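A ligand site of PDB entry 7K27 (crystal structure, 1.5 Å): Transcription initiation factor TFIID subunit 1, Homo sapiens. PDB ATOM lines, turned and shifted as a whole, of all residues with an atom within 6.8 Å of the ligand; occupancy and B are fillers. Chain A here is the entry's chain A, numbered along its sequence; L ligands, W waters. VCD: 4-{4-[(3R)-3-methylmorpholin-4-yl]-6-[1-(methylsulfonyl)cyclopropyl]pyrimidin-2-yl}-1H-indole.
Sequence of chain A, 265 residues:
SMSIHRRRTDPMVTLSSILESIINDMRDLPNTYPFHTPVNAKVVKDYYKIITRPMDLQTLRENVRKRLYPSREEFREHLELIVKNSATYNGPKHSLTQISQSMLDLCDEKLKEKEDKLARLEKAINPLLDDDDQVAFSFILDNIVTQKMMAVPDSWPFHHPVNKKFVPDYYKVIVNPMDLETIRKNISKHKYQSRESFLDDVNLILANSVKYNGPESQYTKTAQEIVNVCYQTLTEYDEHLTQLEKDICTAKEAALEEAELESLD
O of Pro 161 sits close to O26 of the ligand.
Trp 156 touches the ligand.
Pro 157 touches the ligand.
Phe 158 touches the ligand (CE1 to C11, 3.6 Å).
O of His 160 touches C28 of the ligand, 3.2 Å away.
Val 162 touches the ligand.
CB of Phe 166 touches C16 of the ligand (3.8 Å).
Val 167 touches the ligand.
CE2 of Tyr 212 touches C13 of the ligand, at 3.7 Å.
OH of Tyr 219 touches C21 of the ligand (3.3 Å).
Hydrophobic or aromatic side chains within 4 Å of the ligand: Trp 156, Pro 157, Phe 158, Val 162, Phe 166, Val 167, Tyr 212 and Tyr 219.
12 residues have an atom within 4 Å of the ligand: Trp 156, Pro 157, Phe 158, His 160, Pro 161, Val 162, Asn 163, Phe 166, Val 167, Tyr 212, Asn 213 and Tyr 219.
The nearest printed residue that does not touch the ligand is Tyr 170 (4.4 Å).
An oxygen (O10) of the ligand is in hydrogen-bond range of the side-chain amide nitrogen (ND2) of Asn 213 (2.9 Å).
The backbone NH (N) of Asn 163 sits at hydrogen-bond distance from an oxygen (O27) of the ligand (2.9 Å).
The side-chain hydroxyl of Ser 217 is in hydrogen-bond range of the backbone NH of Tyr 219 (3.0 Å).
The backbone NH (N) of Lys 165 is in hydrogen-bond range of the side-chain amide oxygen (OD1) of Asn 163, at 2.9 Å.
The side-chain amide nitrogen (ND2) of Asn 213 lies within hydrogen-bond range of the side-chain hydroxyl (OG) of Ser 209 (3.0 Å).
Water W2 lies within hydrogen-bond range of O of Pro 161 and O26 of the ligand.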
ATOM      1  N   TRP A 156     -18.639 -28.054 -13.479  1.00  0.00           N
ATOM      2  CA  TRP A 156     -19.495 -27.498 -12.435  1.00  0.00           C
ATOM      3  C   TRP A 156     -18.818 -26.467 -11.535  1.00  0.00           C
ATOM      4  O   TRP A 156     -19.496 -25.522 -11.104  1.00  0.00           O
ATOM      5  CB  TRP A 156     -20.125 -28.624 -11.582  1.00  0.00           C
ATOM      6  CG  TRP A 156     -19.134 -29.416 -10.798  1.00  0.00           C
ATOM      7  CD1 TRP A 156     -18.521 -30.587 -11.161  1.00  0.00           C
ATOM      8  CD2 TRP A 156     -18.642 -29.088  -9.504  1.00  0.00           C
ATOM      9  NE1 TRP A 156     -17.623 -30.954 -10.193  1.00  0.00           N
ATOM     10  CE2 TRP A 156     -17.700 -30.070  -9.159  1.00  0.00           C
ATOM     11  CE3 TRP A 156     -18.906 -28.037  -8.585  1.00  0.00           C
ATOM     12  CZ2 TRP A 156     -16.991 -30.049  -7.951  1.00  0.00           C
ATOM     13  CZ3 TRP A 156     -18.195 -28.033  -7.375  1.00  0.00           C
ATOM     14  CH2 TRP A 156     -17.240 -28.985  -7.099  1.00  0.00           C
ATOM     15  N   PRO A 157     -17.515 -26.566 -11.198  1.00  0.00           N
ATOM     16  CA  PRO A 157     -16.963 -25.561 -10.282  1.00  0.00           C
ATOM     17  C   PRO A 157     -17.061 -24.164 -10.817  1.00  0.00           C
ATOM     18  O   PRO A 157     -16.976 -23.201 -10.045  1.00  0.00           O
ATOM     19  CB  PRO A 157     -15.512 -26.000 -10.088  1.00  0.00           C
ATOM     20  CG  PRO A 157     -15.524 -27.496 -10.408  1.00  0.00           C
ATOM     21  CD  PRO A 157     -16.491 -27.584 -11.540  1.00  0.00           C
ATOM     22  N   PHE A 158     -17.185 -24.027 -12.139  1.00  0.00           N
ATOM     23  CA  PHE A 158     -17.161 -22.757 -12.835  1.00  0.00           C
ATOM     24  C   PHE A 158     -18.545 -22.313 -13.272  1.00  0.00           C
ATOM     25  O   PHE A 158     -18.657 -21.239 -13.873  1.00  0.00           O
ATOM     26  CB  PHE A 158     -16.212 -22.864 -14.041  1.00  0.00           C
ATOM     27  CG  PHE A 158     -14.881 -23.410 -13.672  1.00  0.00           C
ATOM     28  CD1 PHE A 158     -14.002 -22.624 -12.928  1.00  0.00           C
ATOM     29  CD2 PHE A 158     -14.469 -24.702 -13.999  1.00  0.00           C
ATOM     30  CE1 PHE A 158     -12.768 -23.114 -12.537  1.00  0.00           C
ATOM     31  CE2 PHE A 158     -13.241 -25.189 -13.586  1.00  0.00           C
ATOM     32  CZ  PHE A 158     -12.377 -24.359 -12.848  1.00  0.00           C
ATOM     33  N   HIS A 159     -19.593 -23.031 -12.909  1.00  0.00           N
ATOM     34  CA  HIS A 159     -20.906 -22.666 -13.400  1.00  0.00           C
ATOM     35  C   HIS A 159     -21.538 -21.533 -12.604  1.00  0.00           C
ATOM     36  O   HIS A 159     -22.457 -20.905 -13.116  1.00  0.00           O
ATOM     37  CB  HIS A 159     -21.849 -23.882 -13.335  1.00  0.00           C
ATOM     38  CG  HIS A 159     -21.607 -24.903 -14.397  1.00  0.00           C
ATOM     39  ND1 HIS A 159     -22.597 -25.772 -14.809  1.00  0.00           N
ATOM     40  CD2 HIS A 159     -20.519 -25.184 -15.145  1.00  0.00           C
ATOM     41  CE1 HIS A 159     -22.106 -26.556 -15.765  1.00  0.00           C
ATOM     42  NE2 HIS A 159     -20.855 -26.207 -15.995  1.00  0.00           N
ATOM     43  N   HIS A 160     -21.105 -21.284 -11.375  1.00  0.00           N
ATOM     44  CA  HIS A 160     -21.780 -20.351 -10.471  1.00  0.00           C
ATOM     45  C   HIS A 160     -20.732 -19.680  -9.640  1.00  0.00           C
ATOM     46  O   HIS A 160     -19.624 -20.203  -9.494  1.00  0.00           O
ATOM     47  CB  HIS A 160     -22.773 -21.034  -9.524  1.00  0.00           C
ATOM     48  CG  HIS A 160     -23.814 -21.803 -10.222  1.00  0.00           C
ATOM     49  ND1 HIS A 160     -24.931 -21.198 -10.781  1.00  0.00           N
ATOM     50  CD2 HIS A 160     -23.925 -23.113 -10.490  1.00  0.00           C
ATOM     51  CE1 HIS A 160     -25.678 -22.124 -11.356  1.00  0.00           C
ATOM     52  NE2 HIS A 160     -25.095 -23.289 -11.189  1.00  0.00           N
ATOM     53  N   PRO A 161     -21.050 -18.533  -9.021  1.00  0.00           N
ATOM     54  CA  PRO A 161     -20.114 -17.943  -8.068  1.00  0.00           C
ATOM     55  C   PRO A 161     -19.838 -18.896  -6.909  1.00  0.00           C
ATOM     56  O   PRO A 161     -20.732 -19.611  -6.453  1.00  0.00           O
ATOM     57  CB  PRO A 161     -20.838 -16.682  -7.561  1.00  0.00           C
ATOM     58  CG  PRO A 161     -21.932 -16.450  -8.506  1.00  0.00           C
ATOM     59  CD  PRO A 161     -22.274 -17.772  -9.145  1.00  0.00           C
ATOM     60  N   VAL A 162     -18.585 -18.890  -6.448  1.00  0.00           N
ATOM     61  CA  VAL A 162     -18.254 -19.710  -5.282  1.00  0.00           C
ATOM     62  C   VAL A 162     -19.050 -19.205  -4.085  1.00  0.00           C
ATOM     63  O   VAL A 162     -19.137 -18.003  -3.808  1.00  0.00           O
ATOM     64  CB  VAL A 162     -16.749 -19.632  -4.993  1.00  0.00           C
ATOM     65  CG1 VAL A 162     -16.411 -20.240  -3.682  1.00  0.00           C
ATOM     66  CG2 VAL A 162     -16.002 -20.341  -6.109  1.00  0.00           C
ATOM     67  N   ASN A 163     -19.588 -20.146  -3.320  1.00  0.00           N
ATOM     68  CA  ASN A 163     -20.255 -19.811  -2.074  1.00  0.00           C
ATOM     69  C   ASN A 163     -19.208 -19.888  -0.964  1.00  0.00           C
ATOM     70  O   ASN A 163     -18.668 -20.950  -0.666  1.00  0.00           O
ATOM     71  CB  ASN A 163     -21.399 -20.782  -1.764  1.00  0.00           C
ATOM     72  CG  ASN A 163     -22.248 -20.304  -0.637  1.00  0.00           C
ATOM     73  OD1 ASN A 163     -21.765 -19.708   0.322  1.00  0.00           O
ATOM     74  ND2 ASN A 163     -23.562 -20.489  -0.749  1.00  0.00           N
ATOM     75  N   LYS A 164     -18.891 -18.747  -0.360  1.00  0.00           N
ATOM     76  CA  LYS A 164     -17.887 -18.654   0.678  1.00  0.00           C
ATOM     77  C   LYS A 164     -18.187 -19.587   1.850  1.00  0.00           C
ATOM     78  O   LYS A 164     -17.293 -19.964   2.574  1.00  0.00           O
ATOM     79  CB  LYS A 164     -17.759 -17.169   1.104  1.00  0.00           C
ATOM     80  CG  LYS A 164     -16.570 -16.913   2.028  1.00  0.00           C
ATOM     81  CD  LYS A 164     -16.197 -15.417   2.028  1.00  0.00           C
ATOM     82  CE  LYS A 164     -17.263 -14.693   2.663  1.00  0.00           C
ATOM     83  NZ  LYS A 164     -16.877 -13.195   2.697  1.00  0.00           N
ATOM     84  N   LYS A 165     -19.453 -19.949   2.085  1.00  0.00           N
ATOM     85  CA  LYS A 165     -19.714 -20.894   3.167  1.00  0.00           C
ATOM     86  C   LYS A 165     -18.990 -22.204   2.933  1.00  0.00           C
ATOM     87  O   LYS A 165     -18.579 -22.887   3.890  1.00  0.00           O
ATOM     88  CB  LYS A 165     -21.217 -21.143   3.290  1.00  0.00           C
ATOM     89  CG  LYS A 165     -21.613 -21.963   4.499  1.00  0.00           C
ATOM     90  CD  LYS A 165     -23.126 -22.107   4.587  1.00  0.00           C
ATOM     91  CE  LYS A 165     -23.555 -22.646   5.929  1.00  0.00           C
ATOM     92  NZ  LYS A 165     -25.022 -22.873   5.895  1.00  0.00           N
ATOM     93  N   PHE A 166     -18.895 -22.610   1.689  1.00  0.00           N
ATOM     94  CA  PHE A 166     -18.319 -23.890   1.345  1.00  0.00           C
ATOM     95  C   PHE A 166     -16.849 -23.827   1.010  1.00  0.00           C
ATOM     96  O   PHE A 166     -16.160 -24.861   1.075  1.00  0.00           O
ATOM     97  CB  PHE A 166     -19.049 -24.504   0.149  1.00  0.00           C
ATOM     98  CG  PHE A 166     -20.517 -24.685   0.353  1.00  0.00           C
ATOM     99  CD1 PHE A 166     -21.044 -25.083   1.569  1.00  0.00           C
ATOM    100  CD2 PHE A 166     -21.398 -24.463  -0.699  1.00  0.00           C
ATOM    101  CE1 PHE A 166     -22.443 -25.233   1.770  1.00  0.00           C
ATOM    102  CE2 PHE A 166     -22.770 -24.607  -0.522  1.00  0.00           C
ATOM    103  CZ  PHE A 166     -23.282 -24.973   0.698  1.00  0.00           C
ATOM    104  N   VAL A 167     -16.343 -22.664   0.631  1.00  0.00           N
ATOM    105  CA  VAL A 167     -14.930 -22.444   0.320  1.00  0.00           C
ATOM    106  C   VAL A 167     -14.501 -21.179   1.069  1.00  0.00           C
ATOM    107  O   VAL A 167     -14.434 -20.079   0.505  1.00  0.00           O
ATOM    108  CB  VAL A 167     -14.692 -22.336  -1.188  1.00  0.00           C
ATOM    109  CG1 VAL A 167     -13.175 -22.384  -1.481  1.00  0.00           C
ATOM    110  CG2 VAL A 167     -15.434 -23.444  -1.979  1.00  0.00           C
ATOM    111  N   TYR A 170     -11.922 -18.456  -0.336  1.00  0.00           N
ATOM    112  CA  TYR A 170     -11.851 -18.250  -1.777  1.00  0.00           C
ATOM    113  C   TYR A 170     -11.650 -16.780  -2.137  1.00  0.00           C
ATOM    114  O   TYR A 170     -10.843 -16.430  -3.020  1.00  0.00           O
ATOM    115  CB  TYR A 170     -13.110 -18.768  -2.466  1.00  0.00           C
ATOM    116  CG  TYR A 170     -12.997 -18.722  -3.966  1.00  0.00           C
ATOM    117  CD1 TYR A 170     -12.227 -19.641  -4.636  1.00  0.00           C
ATOM    118  CD2 TYR A 170     -13.592 -17.696  -4.697  1.00  0.00           C
ATOM    119  CE1 TYR A 170     -12.082 -19.568  -6.016  1.00  0.00           C
ATOM    120  CE2 TYR A 170     -13.492 -17.653  -6.080  1.00  0.00           C
ATOM    121  CZ  TYR A 170     -12.710 -18.589  -6.698  1.00  0.00           C
ATOM    122  OH  TYR A 170     -12.590 -18.491  -8.083  1.00  0.00           O
ATOM    123  N   ASP A 179     -17.542 -16.289 -13.182  1.00  0.00           N
ATOM    124  CA  ASP A 179     -18.091 -17.619 -13.367  1.00  0.00           C
ATOM    125  C   ASP A 179     -19.069 -17.556 -14.537  1.00  0.00           C
ATOM    126  O   ASP A 179     -19.434 -16.479 -15.012  1.00  0.00           O
ATOM    127  CB  ASP A 179     -18.805 -18.078 -12.095  1.00  0.00           C
ATOM    128  CG  ASP A 179     -19.994 -17.233 -11.828  1.00  0.00           C
ATOM    129  OD1 ASP A 179     -19.827 -16.140 -11.212  1.00  0.00           O
ATOM    130  OD2 ASP A 179     -21.093 -17.546 -12.329  1.00  0.00           O
ATOM    131  N   ASN A 208      -8.378 -17.048 -12.587  1.00  0.00           N
ATOM    132  CA  ASN A 208      -8.672 -17.299 -11.197  1.00  0.00           C
ATOM    133  C   ASN A 208      -8.414 -18.751 -10.819  1.00  0.00           C
ATOM    134  O   ASN A 208      -8.072 -19.034  -9.671  1.00  0.00           O
ATOM    135  CB  ASN A 208     -10.107 -16.916 -10.881  1.00  0.00           C
ATOM    136  CG  ASN A 208     -10.284 -15.404 -10.941  1.00  0.00           C
ATOM    137  OD1 ASN A 208      -9.338 -14.657 -10.797  1.00  0.00           O
ATOM    138  ND2 ASN A 208     -11.513 -14.976 -11.102  1.00  0.00           N
ATOM    139  N   SER A 209      -8.634 -19.691 -11.747  1.00  0.00           N
ATOM    140  CA  SER A 209      -8.302 -21.078 -11.419  1.00  0.00           C
ATOM    141  C   SER A 209      -6.807 -21.298 -11.293  1.00  0.00           C
ATOM    142  O   SER A 209      -6.348 -22.004 -10.396  1.00  0.00           O
ATOM    143  CB  SER A 209      -8.881 -22.030 -12.475  1.00  0.00           C
ATOM    144  OG  SER A 209      -8.683 -23.376 -12.113  1.00  0.00           O
ATOM    145  N   TYR A 212      -5.998 -19.815  -7.776  1.00  0.00           N
ATOM    146  CA  TYR A 212      -6.545 -20.475  -6.586  1.00  0.00           C
ATOM    147  C   TYR A 212      -6.144 -21.941  -6.535  1.00  0.00           C
ATOM    148  O   TYR A 212      -5.774 -22.461  -5.476  1.00  0.00           O
ATOM    149  CB  TYR A 212      -8.086 -20.334  -6.502  1.00  0.00           C
ATOM    150  CG  TYR A 212      -8.604 -20.866  -5.191  1.00  0.00           C
ATOM    151  CD1 TYR A 212      -8.535 -20.089  -4.044  1.00  0.00           C
ATOM    152  CD2 TYR A 212      -9.090 -22.142  -5.076  1.00  0.00           C
ATOM    153  CE1 TYR A 212      -8.914 -20.574  -2.825  1.00  0.00           C
ATOM    154  CE2 TYR A 212      -9.510 -22.644  -3.857  1.00  0.00           C
ATOM    155  CZ  TYR A 212      -9.421 -21.868  -2.730  1.00  0.00           C
ATOM    156  OH  TYR A 212      -9.802 -22.336  -1.485  1.00  0.00           O
ATOM    157  N   ASN A 213      -6.160 -22.614  -7.674  1.00  0.00           N
ATOM    158  CA  ASN A 213      -5.945 -24.054  -7.730  1.00  0.00           C
ATOM    159  C   ASN A 213      -4.561 -24.442  -8.196  1.00  0.00           C
ATOM    160  O   ASN A 213      -4.114 -25.559  -7.898  1.00  0.00           O
ATOM    161  CB  ASN A 213      -6.957 -24.672  -8.686  1.00  0.00           C
ATOM    162  CG  ASN A 213      -8.377 -24.418  -8.279  1.00  0.00           C
ATOM    163  OD1 ASN A 213      -8.760 -24.717  -7.145  1.00  0.00           O
ATOM    164  ND2 ASN A 213      -9.186 -23.860  -9.178  1.00  0.00           N
ATOM    165  N   SER A 217      -3.456 -28.066 -11.753  1.00  0.00           N
ATOM    166  CA  SER A 217      -4.644 -28.673 -11.146  1.00  0.00           C
ATOM    167  C   SER A 217      -5.573 -29.219 -12.215  1.00  0.00           C
ATOM    168  O   SER A 217      -5.696 -28.640 -13.300  1.00  0.00           O
ATOM    169  CB  SER A 217      -5.357 -27.603 -10.307  1.00  0.00           C
ATOM    170  OG  SER A 217      -6.691 -27.942  -9.841  1.00  0.00           O
ATOM    171  N   TYR A 219      -8.677 -28.806 -11.907  1.00  0.00           N
ATOM    172  CA  TYR A 219      -9.631 -27.695 -12.062  1.00  0.00           C
ATOM    173  C   TYR A 219      -9.160 -26.753 -13.153  1.00  0.00           C
ATOM    174  O   TYR A 219      -9.942 -26.305 -13.990  1.00  0.00           O
ATOM    175  CB  TYR A 219      -9.790 -26.941 -10.722  1.00  0.00           C
ATOM    176  CG  TYR A 219     -10.523 -27.745  -9.689  1.00  0.00           C
ATOM    177  CD1 TYR A 219     -10.075 -27.785  -8.399  1.00  0.00           C
ATOM    178  CD2 TYR A 219     -11.717 -28.388 -10.016  1.00  0.00           C
ATOM    179  CE1 TYR A 219     -10.750 -28.566  -7.440  1.00  0.00           C
ATOM    180  CE2 TYR A 219     -12.382 -29.168  -9.067  1.00  0.00           C
ATOM    181  CZ  TYR A 219     -11.900 -29.207  -7.793  1.00  0.00           C
ATOM    182  OH  TYR A 219     -12.573 -30.004  -6.831  1.00  0.00           O
HETATM  183  C11 VCD L   1     -13.095 -23.251  -8.985  1.00  0.00           C
HETATM  184  C01 VCD L   1     -16.769 -23.910  -6.797  1.00  0.00           C
HETATM  185  C02 VCD L   1     -17.922 -24.290  -6.108  1.00  0.00           C
HETATM  186  C04 VCD L   1     -16.674 -25.821  -4.807  1.00  0.00           C
HETATM  187  C06 VCD L   1     -15.557 -24.552  -6.472  1.00  0.00           C
HETATM  188  C08 VCD L   1     -13.097 -24.789  -6.522  1.00  0.00           C
HETATM  189  C09 VCD L   1     -12.046 -24.863  -7.659  1.00  0.00           C
HETATM  190  C12 VCD L   1     -14.234 -23.084  -7.952  1.00  0.00           C
HETATM  191  C13 VCD L   1     -12.589 -23.937  -5.351  1.00  0.00           C
HETATM  192  C14 VCD L   1     -16.591 -26.755  -3.752  1.00  0.00           C
HETATM  193  C15 VCD L   1     -17.462 -26.645  -2.678  1.00  0.00           C
HETATM  194  C16 VCD L   1     -17.432 -27.532  -1.560  1.00  0.00           C
HETATM  195  C17 VCD L   1     -16.441 -28.534  -1.514  1.00  0.00           C
HETATM  196  C18 VCD L   1     -15.547 -28.652  -2.585  1.00  0.00           C
HETATM  197  C19 VCD L   1     -15.591 -27.787  -3.717  1.00  0.00           C
HETATM  198  C20 VCD L   1     -14.581 -28.182  -4.576  1.00  0.00           C
HETATM  199  C21 VCD L   1     -13.952 -29.263  -3.969  1.00  0.00           C
HETATM  200  C23 VCD L   1     -19.261 -23.704  -6.418  1.00  0.00           C
HETATM  201  C25 VCD L   1     -20.896 -25.196  -4.559  1.00  0.00           C
HETATM  202  C28 VCD L   1     -19.470 -22.656  -7.495  1.00  0.00           C
HETATM  203  C29 VCD L   1     -19.953 -24.086  -7.728  1.00  0.00           C
HETATM  204  N03 VCD L   1     -17.842 -25.226  -5.126  1.00  0.00           N
HETATM  205  N05 VCD L   1     -15.546 -25.463  -5.470  1.00  0.00           N
HETATM  206  N07 VCD L   1     -14.355 -24.253  -7.089  1.00  0.00           N
HETATM  207  N22 VCD L   1     -14.539 -29.506  -2.801  1.00  0.00           N
HETATM  208  O10 VCD L   1     -11.897 -23.578  -8.301  1.00  0.00           O
HETATM  209  O26 VCD L   1     -21.533 -22.782  -5.508  1.00  0.00           O
HETATM  210  O27 VCD L   1     -19.559 -22.980  -3.845  1.00  0.00           O
HETATM  211  S24 VCD L   1     -20.349 -23.543  -5.014  1.00  0.00           S
HETATM  212  O   HOH W   1     -12.658 -30.644  -1.030  1.00  0.00           O
HETATM  213  O   HOH W   2     -22.992 -19.690  -5.046  1.00  0.00           O
HETATM  214  O   HOH W   3     -22.046 -25.703  -9.941  1.00  0.00           O
